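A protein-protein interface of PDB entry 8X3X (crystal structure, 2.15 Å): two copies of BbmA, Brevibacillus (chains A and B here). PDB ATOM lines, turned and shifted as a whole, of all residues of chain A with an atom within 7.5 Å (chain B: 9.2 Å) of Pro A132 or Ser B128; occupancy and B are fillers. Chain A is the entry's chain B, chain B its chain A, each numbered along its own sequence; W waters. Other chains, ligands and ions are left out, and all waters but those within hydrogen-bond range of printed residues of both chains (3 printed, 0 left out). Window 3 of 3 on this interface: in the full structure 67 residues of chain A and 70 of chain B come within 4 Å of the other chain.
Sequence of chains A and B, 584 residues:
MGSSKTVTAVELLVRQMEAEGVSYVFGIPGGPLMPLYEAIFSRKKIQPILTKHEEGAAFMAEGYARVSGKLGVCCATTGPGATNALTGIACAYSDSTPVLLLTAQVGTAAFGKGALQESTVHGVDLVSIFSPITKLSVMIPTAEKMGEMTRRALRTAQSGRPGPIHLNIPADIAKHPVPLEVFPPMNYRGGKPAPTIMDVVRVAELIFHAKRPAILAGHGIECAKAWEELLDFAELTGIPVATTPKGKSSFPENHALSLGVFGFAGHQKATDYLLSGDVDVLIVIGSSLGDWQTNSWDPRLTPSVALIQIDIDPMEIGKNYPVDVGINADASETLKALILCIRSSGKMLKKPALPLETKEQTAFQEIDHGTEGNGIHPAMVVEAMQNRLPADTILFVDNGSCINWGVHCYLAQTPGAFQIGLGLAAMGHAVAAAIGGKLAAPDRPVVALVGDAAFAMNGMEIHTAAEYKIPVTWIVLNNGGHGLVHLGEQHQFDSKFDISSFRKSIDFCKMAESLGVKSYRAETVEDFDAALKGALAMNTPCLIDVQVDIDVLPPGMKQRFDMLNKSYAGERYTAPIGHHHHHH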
ATOM      1  N   LEU A  86      16.832 -14.143  17.152  1.00  0.00           N
ATOM      2  CA  LEU A  86      16.062 -14.874  16.149  1.00  0.00           C
ATOM      3  C   LEU A  86      15.760 -14.033  14.918  1.00  0.00           C
ATOM      4  O   LEU A  86      15.889 -14.513  13.784  1.00  0.00           O
ATOM      5  CB  LEU A  86      14.759 -15.393  16.752  1.00  0.00           C
ATOM      6  CG  LEU A  86      14.028 -16.267  15.739  1.00  0.00           C
ATOM      7  CD1 LEU A  86      14.284 -17.722  16.083  1.00  0.00           C
ATOM      8  CD2 LEU A  86      12.556 -15.941  15.795  1.00  0.00           C
ATOM      9  N   TYR A  93      18.223 -16.084   6.900  1.00  0.00           N
ATOM     10  CA  TYR A  93      17.520 -17.149   6.201  1.00  0.00           C
ATOM     11  C   TYR A  93      16.808 -16.611   4.960  1.00  0.00           C
ATOM     12  O   TYR A  93      16.910 -17.186   3.870  1.00  0.00           O
ATOM     13  CB  TYR A  93      16.549 -17.801   7.184  1.00  0.00           C
ATOM     14  CG  TYR A  93      15.773 -18.974   6.656  1.00  0.00           C
ATOM     15  CD1 TYR A  93      16.350 -20.242   6.585  1.00  0.00           C
ATOM     16  CD2 TYR A  93      14.444 -18.826   6.266  1.00  0.00           C
ATOM     17  CE1 TYR A  93      15.617 -21.342   6.113  1.00  0.00           C
ATOM     18  CE2 TYR A  93      13.712 -19.900   5.806  1.00  0.00           C
ATOM     19  CZ  TYR A  93      14.303 -21.153   5.726  1.00  0.00           C
ATOM     20  OH  TYR A  93      13.564 -22.210   5.267  1.00  0.00           O
ATOM     21  N   LEU A 126      15.421 -24.231  22.224  1.00  0.00           N
ATOM     22  CA  LEU A 126      16.065 -23.405  21.196  1.00  0.00           C
ATOM     23  C   LEU A 126      16.255 -24.164  19.877  1.00  0.00           C
ATOM     24  O   LEU A 126      16.128 -23.585  18.793  1.00  0.00           O
ATOM     25  CB  LEU A 126      17.419 -22.891  21.705  1.00  0.00           C
ATOM     26  CG  LEU A 126      17.459 -21.955  22.931  1.00  0.00           C
ATOM     27  CD1 LEU A 126      18.910 -21.678  23.342  1.00  0.00           C
ATOM     28  CD2 LEU A 126      16.734 -20.645  22.650  1.00  0.00           C
ATOM     29  N   VAL A 127      16.589 -25.449  19.948  1.00  0.00           N
ATOM     30  CA  VAL A 127      16.810 -26.206  18.726  1.00  0.00           C
ATOM     31  C   VAL A 127      15.556 -26.196  17.862  1.00  0.00           C
ATOM     32  O   VAL A 127      15.624 -25.954  16.647  1.00  0.00           O
ATOM     33  CB  VAL A 127      17.280 -27.635  19.068  1.00  0.00           C
ATOM     34  CG1 VAL A 127      17.143 -28.564  17.836  1.00  0.00           C
ATOM     35  CG2 VAL A 127      18.716 -27.567  19.542  1.00  0.00           C
ATOM     36  N   SER A 128      14.386 -26.428  18.487  1.00  0.00           N
ATOM     37  CA  SER A 128      13.105 -26.426  17.783  1.00  0.00           C
ATOM     38  C   SER A 128      12.704 -25.024  17.335  1.00  0.00           C
ATOM     39  O   SER A 128      12.156 -24.854  16.245  1.00  0.00           O
ATOM     40  CB  SER A 128      12.007 -27.014  18.688  1.00  0.00           C
ATOM     41  OG  SER A 128      12.262 -28.382  18.959  1.00  0.00           O
ATOM     42  N   ILE A 129      12.931 -24.009  18.174  1.00  0.00           N
ATOM     43  CA  ILE A 129      12.544 -22.649  17.799  1.00  0.00           C
ATOM     44  C   ILE A 129      13.283 -22.204  16.540  1.00  0.00           C
ATOM     45  O   ILE A 129      12.718 -21.518  15.671  1.00  0.00           O
ATOM     46  CB  ILE A 129      12.794 -21.671  18.963  1.00  0.00           C
ATOM     47  CG1 ILE A 129      11.796 -21.898  20.105  1.00  0.00           C
ATOM     48  CG2 ILE A 129      12.717 -20.248  18.464  1.00  0.00           C
ATOM     49  CD1 ILE A 129      12.173 -21.176  21.428  1.00  0.00           C
ATOM     50  N   PHE A 130      14.557 -22.583  16.420  1.00  0.00           N
ATOM     51  CA  PHE A 130      15.377 -22.165  15.285  1.00  0.00           C
ATOM     52  C   PHE A 130      15.253 -23.078  14.065  1.00  0.00           C
ATOM     53  O   PHE A 130      15.609 -22.658  12.960  1.00  0.00           O
ATOM     54  CB  PHE A 130      16.855 -22.056  15.718  1.00  0.00           C
ATOM     55  CG  PHE A 130      17.182 -20.732  16.340  1.00  0.00           C
ATOM     56  CD1 PHE A 130      17.011 -20.538  17.699  1.00  0.00           C
ATOM     57  CD2 PHE A 130      17.572 -19.652  15.551  1.00  0.00           C
ATOM     58  CE1 PHE A 130      17.271 -19.314  18.272  1.00  0.00           C
ATOM     59  CE2 PHE A 130      17.829 -18.424  16.111  1.00  0.00           C
ATOM     60  CZ  PHE A 130      17.676 -18.251  17.481  1.00  0.00           C
ATOM     61  N   SER A 131      14.732 -24.294  14.215  1.00  0.00           N
ATOM     62  CA  SER A 131      14.641 -25.191  13.062  1.00  0.00           C
ATOM     63  C   SER A 131      13.977 -24.572  11.829  1.00  0.00           C
ATOM     64  O   SER A 131      14.492 -24.783  10.721  1.00  0.00           O
ATOM     65  CB  SER A 131      13.905 -26.476  13.470  1.00  0.00           C
ATOM     66  OG  SER A 131      14.791 -27.343  14.137  1.00  0.00           O
ATOM     67  N   PRO A 132      12.860 -23.834  11.923  1.00  0.00           N
ATOM     68  CA  PRO A 132      12.220 -23.321  10.692  1.00  0.00           C
ATOM     69  C   PRO A 132      13.015 -22.258   9.945  1.00  0.00           C
ATOM     70  O   PRO A 132      12.714 -22.036   8.770  1.00  0.00           O
ATOM     71  CB  PRO A 132      10.892 -22.731  11.196  1.00  0.00           C
ATOM     72  CG  PRO A 132      10.654 -23.421  12.539  1.00  0.00           C
ATOM     73  CD  PRO A 132      12.029 -23.610  13.118  1.00  0.00           C
ATOM     74  N   ILE A 133      13.983 -21.566  10.568  1.00  0.00           N
ATOM     75  CA  ILE A 133      14.659 -20.467   9.874  1.00  0.00           C
ATOM     76  C   ILE A 133      16.169 -20.674   9.850  1.00  0.00           C
ATOM     77  O   ILE A 133      16.942 -19.706   9.832  1.00  0.00           O
ATOM     78  CB  ILE A 133      14.301 -19.098  10.492  1.00  0.00           C
ATOM     79  CG1 ILE A 133      14.259 -19.150  12.027  1.00  0.00           C
ATOM     80  CG2 ILE A 133      12.931 -18.666   9.999  1.00  0.00           C
ATOM     81  CD1 ILE A 133      15.569 -19.051  12.721  1.00  0.00           C
ATOM     82  N   THR A 134      16.601 -21.934   9.846  1.00  0.00           N
ATOM     83  CA  THR A 134      18.006 -22.272   9.647  1.00  0.00           C
ATOM     84  C   THR A 134      18.059 -23.465   8.712  1.00  0.00           C
ATOM     85  O   THR A 134      17.109 -24.246   8.645  1.00  0.00           O
ATOM     86  CB  THR A 134      18.747 -22.666  10.950  1.00  0.00           C
ATOM     87  OG1 THR A 134      17.976 -23.665  11.637  1.00  0.00           O
ATOM     88  CG2 THR A 134      19.047 -21.437  11.882  1.00  0.00           C
ATOM     89  N   LYS A 135      19.181 -23.612   8.003  1.00  0.00           N
ATOM     90  CA  LYS A 135      19.385 -24.832   7.234  1.00  0.00           C
ATOM     91  C   LYS A 135      19.673 -26.011   8.145  1.00  0.00           C
ATOM     92  O   LYS A 135      19.446 -27.157   7.745  1.00  0.00           O
ATOM     93  CB  LYS A 135      20.536 -24.660   6.232  1.00  0.00           C
ATOM     94  CG  LYS A 135      20.314 -23.581   5.189  1.00  0.00           C
ATOM     95  CD  LYS A 135      21.475 -23.529   4.198  1.00  0.00           C
ATOM     96  CE  LYS A 135      21.491 -24.753   3.265  1.00  0.00           C
ATOM     97  NZ  LYS A 135      22.575 -24.574   2.225  1.00  0.00           N
ATOM     98  N   SER A 137      19.755 -26.816  12.640  1.00  0.00           N
ATOM     99  CA  SER A 137      19.639 -26.417  14.043  1.00  0.00           C
ATOM    100  C   SER A 137      19.853 -27.678  14.867  1.00  0.00           C
ATOM    101  O   SER A 137      19.077 -28.630  14.742  1.00  0.00           O
ATOM    102  CB  SER A 137      18.255 -25.809  14.335  1.00  0.00           C
ATOM    103  OG  SER A 137      18.099 -25.476  15.714  1.00  0.00           O
ATOM    104  N   THR B  83       8.720 -12.166  14.904  1.00  0.00           N
ATOM    105  CA  THR B  83       9.926 -12.759  15.498  1.00  0.00           C
ATOM    106  C   THR B  83      10.551 -11.826  16.529  1.00  0.00           C
ATOM    107  O   THR B  83      11.185 -12.295  17.479  1.00  0.00           O
ATOM    108  CB  THR B  83      10.962 -13.144  14.422  1.00  0.00           C
ATOM    109  OG1 THR B  83      11.339 -11.991  13.648  1.00  0.00           O
ATOM    110  CG2 THR B  83      10.396 -14.236  13.492  1.00  0.00           C
ATOM    111  N   LEU B  86       9.386 -12.561  20.160  1.00  0.00           N
ATOM    112  CA  LEU B  86       9.475 -13.931  20.659  1.00  0.00           C
ATOM    113  C   LEU B  86      10.017 -13.987  22.090  1.00  0.00           C
ATOM    114  O   LEU B  86       9.493 -14.722  22.941  1.00  0.00           O
ATOM    115  CB  LEU B  86      10.329 -14.784  19.723  1.00  0.00           C
ATOM    116  CG  LEU B  86      10.271 -16.234  20.217  1.00  0.00           C
ATOM    117  CD1 LEU B  86       9.803 -17.164  19.136  1.00  0.00           C
ATOM    118  CD2 LEU B  86      11.608 -16.669  20.742  1.00  0.00           C
ATOM    119  N   GLN B 105      -0.658 -12.561   8.936  1.00  0.00           N
ATOM    120  CA  GLN B 105      -0.222 -13.519   7.932  1.00  0.00           C
ATOM    121  C   GLN B 105      -0.543 -12.889   6.586  1.00  0.00           C
ATOM    122  O   GLN B 105      -1.438 -12.050   6.500  1.00  0.00           O
ATOM    123  CB  GLN B 105      -0.959 -14.881   8.136  1.00  0.00           C
ATOM    124  CG  GLN B 105      -0.586 -15.981   7.163  1.00  0.00           C
ATOM    125  CD  GLN B 105       0.893 -16.315   7.235  1.00  0.00           C
ATOM    126  OE1 GLN B 105       1.686 -15.797   6.456  1.00  0.00           O
ATOM    127  NE2 GLN B 105       1.271 -17.173   8.184  1.00  0.00           N
ATOM    128  N   GLU B 118       6.421 -13.364   3.840  1.00  0.00           N
ATOM    129  CA  GLU B 118       5.619 -14.579   3.910  1.00  0.00           C
ATOM    130  C   GLU B 118       5.944 -15.350   5.186  1.00  0.00           C
ATOM    131  O   GLU B 118       7.108 -15.644   5.475  1.00  0.00           O
ATOM    132  CB  GLU B 118       5.860 -15.460   2.676  1.00  0.00           C
ATOM    133  CG  GLU B 118       5.002 -16.742   2.704  1.00  0.00           C
ATOM    134  CD  GLU B 118       4.778 -17.367   1.324  1.00  0.00           C
ATOM    135  OE1 GLU B 118       4.208 -18.475   1.273  1.00  0.00           O
ATOM    136  OE2 GLU B 118       5.172 -16.764   0.301  1.00  0.00           O
ATOM    137  N   SER B 119       4.906 -15.670   5.959  1.00  0.00           N
ATOM    138  CA  SER B 119       5.080 -16.226   7.296  1.00  0.00           C
ATOM    139  C   SER B 119       4.503 -17.636   7.412  1.00  0.00           C
ATOM    140  O   SER B 119       4.043 -18.033   8.481  1.00  0.00           O
ATOM    141  CB  SER B 119       4.461 -15.300   8.342  1.00  0.00           C
ATOM    142  OG  SER B 119       5.071 -14.023   8.299  1.00  0.00           O
ATOM    143  N   THR B 120       4.559 -18.404   6.324  1.00  0.00           N
ATOM    144  CA  THR B 120       4.042 -19.762   6.249  1.00  0.00           C
ATOM    145  C   THR B 120       5.184 -20.763   6.303  1.00  0.00           C
ATOM    146  O   THR B 120       6.359 -20.407   6.417  1.00  0.00           O
ATOM    147  CB  THR B 120       3.290 -19.992   4.935  1.00  0.00           C
ATOM    148  OG1 THR B 120       4.244 -19.949   3.853  1.00  0.00           O
ATOM    149  CG2 THR B 120       2.195 -18.947   4.717  1.00  0.00           C
ATOM    150  N   VAL B 121       4.830 -22.036   6.104  1.00  0.00           N
ATOM    151  CA  VAL B 121       5.844 -23.079   5.993  1.00  0.00           C
ATOM    152  C   VAL B 121       6.792 -22.777   4.849  1.00  0.00           C
ATOM    153  O   VAL B 121       7.966 -23.176   4.882  1.00  0.00           O
ATOM    154  CB  VAL B 121       5.180 -24.466   5.826  1.00  0.00           C
ATOM    155  CG1 VAL B 121       4.440 -24.577   4.474  1.00  0.00           C
ATOM    156  CG2 VAL B 121       6.228 -25.584   5.988  1.00  0.00           C
ATOM    157  N   HIS B 122       6.317 -22.042   3.833  1.00  0.00           N
ATOM    158  CA  HIS B 122       7.143 -21.743   2.664  1.00  0.00           C
ATOM    159  C   HIS B 122       8.064 -20.554   2.877  1.00  0.00           C
ATOM    160  O   HIS B 122       8.954 -20.332   2.047  1.00  0.00           O
ATOM    161  CB  HIS B 122       6.262 -21.460   1.432  1.00  0.00           C
ATOM    162  CG  HIS B 122       5.164 -22.462   1.224  1.00  0.00           C
ATOM    163  ND1 HIS B 122       5.409 -23.767   0.853  1.00  0.00           N
ATOM    164  CD2 HIS B 122       3.818 -22.356   1.356  1.00  0.00           C
ATOM    165  CE1 HIS B 122       4.263 -24.418   0.750  1.00  0.00           C
ATOM    166  NE2 HIS B 122       3.282 -23.586   1.052  1.00  0.00           N
ATOM    167  N   GLY B 123       7.837 -19.760   3.926  1.00  0.00           N
ATOM    168  CA  GLY B 123       8.661 -18.603   4.202  1.00  0.00           C
ATOM    169  C   GLY B 123       9.274 -18.684   5.583  1.00  0.00           C
ATOM    170  O   GLY B 123      10.101 -19.563   5.843  1.00  0.00           O
ATOM    171  N   VAL B 124       8.860 -17.782   6.475  1.00  0.00           N
ATOM    172  CA  VAL B 124       9.295 -17.759   7.867  1.00  0.00           C
ATOM    173  C   VAL B 124       8.102 -18.222   8.700  1.00  0.00           C
ATOM    174  O   VAL B 124       7.165 -17.452   8.961  1.00  0.00           O
ATOM    175  CB  VAL B 124       9.784 -16.370   8.293  1.00  0.00           C
ATOM    176  CG1 VAL B 124       9.927 -16.310   9.792  1.00  0.00           C
ATOM    177  CG2 VAL B 124      11.122 -16.029   7.606  1.00  0.00           C
ATOM    178  N   ASP B 125       8.136 -19.486   9.120  1.00  0.00           N
ATOM    179  CA  ASP B 125       6.957 -20.216   9.613  1.00  0.00           C
ATOM    180  C   ASP B 125       6.692 -19.849  11.075  1.00  0.00           C
ATOM    181  O   ASP B 125       7.125 -20.542  11.990  1.00  0.00           O
ATOM    182  CB  ASP B 125       7.183 -21.713   9.448  1.00  0.00           C
ATOM    183  CG  ASP B 125       5.967 -22.542   9.842  1.00  0.00           C
ATOM    184  OD1 ASP B 125       4.989 -21.986  10.386  1.00  0.00           O
ATOM    185  OD2 ASP B 125       6.017 -23.768   9.627  1.00  0.00           O
ATOM    186  N   LEU B 126       5.971 -18.738  11.276  1.00  0.00           N
ATOM    187  CA  LEU B 126       5.665 -18.222  12.613  1.00  0.00           C
ATOM    188  C   LEU B 126       4.980 -19.259  13.491  1.00  0.00           C
ATOM    189  O   LEU B 126       5.311 -19.383  14.672  1.00  0.00           O
ATOM    190  CB  LEU B 126       4.778 -16.975  12.510  1.00  0.00           C
ATOM    191  CG  LEU B 126       5.396 -15.756  11.812  1.00  0.00           C
ATOM    192  CD1 LEU B 126       4.445 -14.539  11.899  1.00  0.00           C
ATOM    193  CD2 LEU B 126       6.771 -15.440  12.431  1.00  0.00           C
ATOM    194  N   VAL B 127       3.999 -19.985  12.954  1.00  0.00           N
ATOM    195  CA  VAL B 127       3.279 -20.939  13.796  1.00  0.00           C
ATOM    196  C   VAL B 127       4.245 -21.960  14.369  1.00  0.00           C
ATOM    197  O   VAL B 127       4.194 -22.278  15.561  1.00  0.00           O
ATOM    198  CB  VAL B 127       2.128 -21.614  13.019  1.00  0.00           C
ATOM    199  CG1 VAL B 127       1.635 -22.865  13.791  1.00  0.00           C
ATOM    200  CG2 VAL B 127       0.983 -20.614  12.804  1.00  0.00           C
ATOM    201  N   SER B 128       5.196 -22.427  13.550  1.00  0.00           N
ATOM    202  CA  SER B 128       6.174 -23.407  14.022  1.00  0.00           C
ATOM    203  C   SER B 128       7.171 -22.778  14.980  1.00  0.00           C
ATOM    204  O   SER B 128       7.584 -23.415  15.955  1.00  0.00           O
ATOM    205  CB  SER B 128       6.930 -24.005  12.849  1.00  0.00           C
ATOM    206  OG  SER B 128       6.130 -24.944  12.182  1.00  0.00           O
ATOM    207  N   ILE B 129       7.608 -21.549  14.694  1.00  0.00           N
ATOM    208  CA  ILE B 129       8.626 -20.904  15.527  1.00  0.00           C
ATOM    209  C   ILE B 129       8.104 -20.725  16.942  1.00  0.00           C
ATOM    210  O   ILE B 129       8.835 -20.911  17.919  1.00  0.00           O
ATOM    211  CB  ILE B 129       9.048 -19.548  14.919  1.00  0.00           C
ATOM    212  CG1 ILE B 129       9.782 -19.763  13.597  1.00  0.00           C
ATOM    213  CG2 ILE B 129       9.870 -18.728  15.936  1.00  0.00           C
ATOM    214  CD1 ILE B 129      10.060 -18.460  12.843  1.00  0.00           C
ATOM    215  N   PHE B 130       6.828 -20.366  17.072  1.00  0.00           N
ATOM    216  CA  PHE B 130       6.243 -20.065  18.366  1.00  0.00           C
ATOM    217  C   PHE B 130       5.724 -21.302  19.077  1.00  0.00           C
ATOM    218  O   PHE B 130       5.470 -21.246  20.283  1.00  0.00           O
ATOM    219  CB  PHE B 130       5.116 -19.039  18.200  1.00  0.00           C
ATOM    220  CG  PHE B 130       5.610 -17.627  18.204  1.00  0.00           C
ATOM    221  CD1 PHE B 130       5.773 -16.934  19.405  1.00  0.00           C
ATOM    222  CD2 PHE B 130       5.976 -17.004  17.017  1.00  0.00           C
ATOM    223  CE1 PHE B 130       6.270 -15.640  19.417  1.00  0.00           C
ATOM    224  CE2 PHE B 130       6.448 -15.712  17.029  1.00  0.00           C
ATOM    225  CZ  PHE B 130       6.601 -15.029  18.222  1.00  0.00           C
ATOM    226  N   SER B 131       5.595 -22.423  18.374  1.00  0.00           N
ATOM    227  CA  SER B 131       4.996 -23.598  18.997  1.00  0.00           C
ATOM    228  C   SER B 131       5.738 -24.045  20.255  1.00  0.00           C
ATOM    229  O   SER B 131       5.071 -24.429  21.227  1.00  0.00           O
ATOM    230  CB  SER B 131       4.899 -24.735  17.969  1.00  0.00           C
ATOM    231  OG  SER B 131       4.105 -25.765  18.493  1.00  0.00           O
ATOM    232  N   PRO B 132       7.065 -23.994  20.335  1.00  0.00           N
ATOM    233  CA  PRO B 132       7.723 -24.476  21.563  1.00  0.00           C
ATOM    234  C   PRO B 132       7.480 -23.612  22.795  1.00  0.00           C
ATOM    235  O   PRO B 132       7.600 -24.134  23.914  1.00  0.00           O
ATOM    236  CB  PRO B 132       9.210 -24.505  21.173  1.00  0.00           C
ATOM    237  CG  PRO B 132       9.161 -24.696  19.656  1.00  0.00           C
ATOM    238  CD  PRO B 132       8.010 -23.870  19.216  1.00  0.00           C
ATOM    239  N   ILE B 133       7.140 -22.326  22.654  1.00  0.00           N
ATOM    240  CA  ILE B 133       7.041 -21.475  23.842  1.00  0.00           C
ATOM    241  C   ILE B 133       5.654 -20.850  23.966  1.00  0.00           C
ATOM    242  O   ILE B 133       5.499 -19.739  24.492  1.00  0.00           O
ATOM    243  CB  ILE B 133       8.145 -20.399  23.848  1.00  0.00           C
ATOM    244  CG1 ILE B 133       8.044 -19.495  22.609  1.00  0.00           C
ATOM    245  CG2 ILE B 133       9.510 -21.065  23.854  1.00  0.00           C
ATOM    246  CD1 ILE B 133       6.783 -18.706  22.535  1.00  0.00           C
ATOM    247  N   THR B 134       4.638 -21.559  23.484  1.00  0.00           N
ATOM    248  CA  THR B 134       3.248 -21.196  23.723  1.00  0.00           C
ATOM    249  C   THR B 134       2.493 -22.457  24.102  1.00  0.00           C
ATOM    250  O   THR B 134       2.920 -23.568  23.772  1.00  0.00           O
ATOM    251  CB  THR B 134       2.591 -20.560  22.491  1.00  0.00           C
ATOM    252  OG1 THR B 134       2.841 -21.393  21.352  1.00  0.00           O
ATOM    253  CG2 THR B 134       3.157 -19.171  22.257  1.00  0.00           C
ATOM    254  N   LEU B 136      -0.412 -22.786  22.838  1.00  0.00           N
ATOM    255  CA  LEU B 136      -1.113 -23.013  21.582  1.00  0.00           C
ATOM    256  C   LEU B 136      -0.571 -22.007  20.578  1.00  0.00           C
ATOM    257  O   LEU B 136      -0.501 -20.811  20.883  1.00  0.00           O
ATOM    258  CB  LEU B 136      -2.631 -22.833  21.747  1.00  0.00           C
ATOM    259  CG  LEU B 136      -3.426 -22.797  20.436  1.00  0.00           C
ATOM    260  CD1 LEU B 136      -3.383 -24.164  19.771  1.00  0.00           C
ATOM    261  CD2 LEU B 136      -4.885 -22.386  20.672  1.00  0.00           C
ATOM    262  N   SER B 137      -0.212 -22.493  19.396  1.00  0.00           N
ATOM    263  CA  SER B 137       0.222 -21.678  18.262  1.00  0.00           C
ATOM    264  C   SER B 137      -0.538 -22.146  17.030  1.00  0.00           C
ATOM    265  O   SER B 137      -0.365 -23.290  16.597  1.00  0.00           O
ATOM    266  CB  SER B 137       1.740 -21.812  18.022  1.00  0.00           C
ATOM    267  OG  SER B 137       2.182 -20.917  16.991  1.00  0.00           O
ATOM    268  N   VAL B 138      -1.344 -21.267  16.438  1.00  0.00           N
ATOM    269  CA  VAL B 138      -2.268 -21.735  15.409  1.00  0.00           C
ATOM    270  C   VAL B 138      -2.619 -20.591  14.475  1.00  0.00           C
ATOM    271  O   VAL B 138      -2.724 -19.428  14.893  1.00  0.00           O
ATOM    272  CB  VAL B 138      -3.531 -22.376  16.054  1.00  0.00           C
ATOM    273  CG1 VAL B 138      -4.389 -21.336  16.723  1.00  0.00           C
ATOM    274  CG2 VAL B 138      -4.319 -23.175  15.006  1.00  0.00           C
ATOM    275  N   MET B 139      -2.788 -20.925  13.195  1.00  0.00           N
ATOM    276  CA  MET B 139      -3.266 -19.977  12.199  1.00  0.00           C
ATOM    277  C   MET B 139      -4.775 -20.148  12.041  1.00  0.00           C
ATOM    278  O   MET B 139      -5.268 -21.277  11.936  1.00  0.00           O
ATOM    279  CB  MET B 139      -2.541 -20.185  10.863  1.00  0.00           C
ATOM    280  CG  MET B 139      -3.022 -19.237   9.743  1.00  0.00           C
ATOM    281  SD  MET B 139      -2.110 -19.450   8.202  1.00  0.00           S
ATOM    282  CE  MET B 139      -3.031 -20.783   7.419  1.00  0.00           C
ATOM    283  N   HIS B 166      -0.247 -17.940  20.673  1.00  0.00           N
ATOM    284  CA  HIS B 166       0.043 -17.281  19.388  1.00  0.00           C
ATOM    285  C   HIS B 166      -1.108 -17.534  18.409  1.00  0.00           C
ATOM    286  O   HIS B 166      -1.374 -18.683  18.044  1.00  0.00           O
ATOM    287  CB  HIS B 166       1.369 -17.791  18.826  1.00  0.00           C
ATOM    288  CG  HIS B 166       1.648 -17.362  17.415  1.00  0.00           C
ATOM    289  ND1 HIS B 166       2.007 -18.257  16.431  1.00  0.00           N
ATOM    290  CD2 HIS B 166       1.603 -16.144  16.818  1.00  0.00           C
ATOM    291  CE1 HIS B 166       2.198 -17.606  15.292  1.00  0.00           C
ATOM    292  NE2 HIS B 166       1.943 -16.325  15.497  1.00  0.00           N
ATOM    293  N   ASN B 168      -2.375 -16.485  14.653  1.00  0.00           N
ATOM    294  CA  ASN B 168      -1.896 -15.948  13.386  1.00  0.00           C
ATOM    295  C   ASN B 168      -3.099 -15.758  12.463  1.00  0.00           C
ATOM    296  O   ASN B 168      -3.891 -16.687  12.262  1.00  0.00           O
ATOM    297  CB  ASN B 168      -0.843 -16.901  12.793  1.00  0.00           C
ATOM    298  CG  ASN B 168      -0.225 -16.392  11.487  1.00  0.00           C
ATOM    299  OD1 ASN B 168      -0.315 -17.060  10.449  1.00  0.00           O
ATOM    300  ND2 ASN B 168       0.434 -15.228  11.539  1.00  0.00           N
HETATM  301  O   HOH W   1      10.249 -21.309   7.876  1.00  0.00           O
HETATM  302  O   HOH W   2      11.045 -21.599   4.170  1.00  0.00           O
HETATM  303  O   HOH W   3       9.483 -25.505  15.759  1.00  0.00           O
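O of Glu B118 is in hydrogen-bond range of N of Val B124 (2.9 Å). The side-chain hydroxyl of Ser B128 sits at hydrogen-bond distance from the side-chain carboxylate of Asp B125 (2.8 Å).
Among the printed residues, pairs that only touch across the chains: Leu A86 with Thr B83 (3.5 Å), Leu A86 with Ile B129 (3.9 Å), Tyr A93 with Gly B123 (3.6 Å), Ser A128 with Pro B132 (3.8 Å), Ile A129 with Ile B129 (3.8 Å), Ile A129 with Pro B132 (3.8 Å), Ile A129 with Ile B133 (3.6 Å), Pro A132 with Ser B128 (3.8 Å), Pro A132 with Ile B129 (3.9 Å) and Ile A133 with Val B124 (3.8 Å).
Ser B128 touches one residue of chain A. Printed residues of chain B within 4 Å of Ile A133: Val B124. Of the printed residues of chain A, Ile B129 touches Leu A86 (3.9 Å), Ile A129 (3.8 Å) and Pro A132 (3.9 Å). Printed residues of chain A within 4 Å of Gly B123: Tyr A93 (3.6 Å). Ser B137 touches none of the printed residues of chain A. The nearest residue of chain A that does not touch Ser B128 is Ser A128 (4.8 Å).
Of the 13 printed residues of chain A, 6 touch a printed residue of chain B. Printed residues of chain A that touch a printed residue of chain B: Leu A86, Tyr A93, Ser A128, Ile A129, Pro A132 and Ile A133. Hydrophobic or aromatic side chains of chain A within 4 Å of the printed part of chain B: Leu A86, Tyr A93, Ile A129, Pro A132 and Ile A133. Of the 26 printed residues of chain B, 7 touch a printed residue of chain A. Hydrophobic or aromatic side chains of chain B within 4 Å of the printed part of chain A: Val B124, Ile B129, Pro B132 and Ile B133.
Leu A86 touches Ile B129, but with the chains exchanged Ile A129 does not touch Leu B86 (4.3 Å). Ser A128 touches Pro B132, and with the chains exchanged Pro A132 touches Ser B128. Ile A129 touches Pro B132, and with the chains exchanged Pro A132 touches Ile B129. Ile A129 touches Ile B133, but with the chains exchanged Ile A133 does not touch Ile B129 (4.05 Å). Positions printed for both chains: 86, 126, 127, 128, 129, 130, 131, 132, 133, 134 and 137. Of the 10 pairs that touch across the chains among the printed residues, 5 have their exchanged pair printed and touching as well.
Water W1 lies within hydrogen-bond range of O of Gly B123 (2.7 Å), O of Pro A132 (2.7 Å) and N of Asp B125 (3.1 Å). Water W3 bridges O of Ser A128 and O of Ser B128. Water W2 lies within hydrogen-bond range of O of Gly B123, OH of Tyr A93 and O of His B122.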
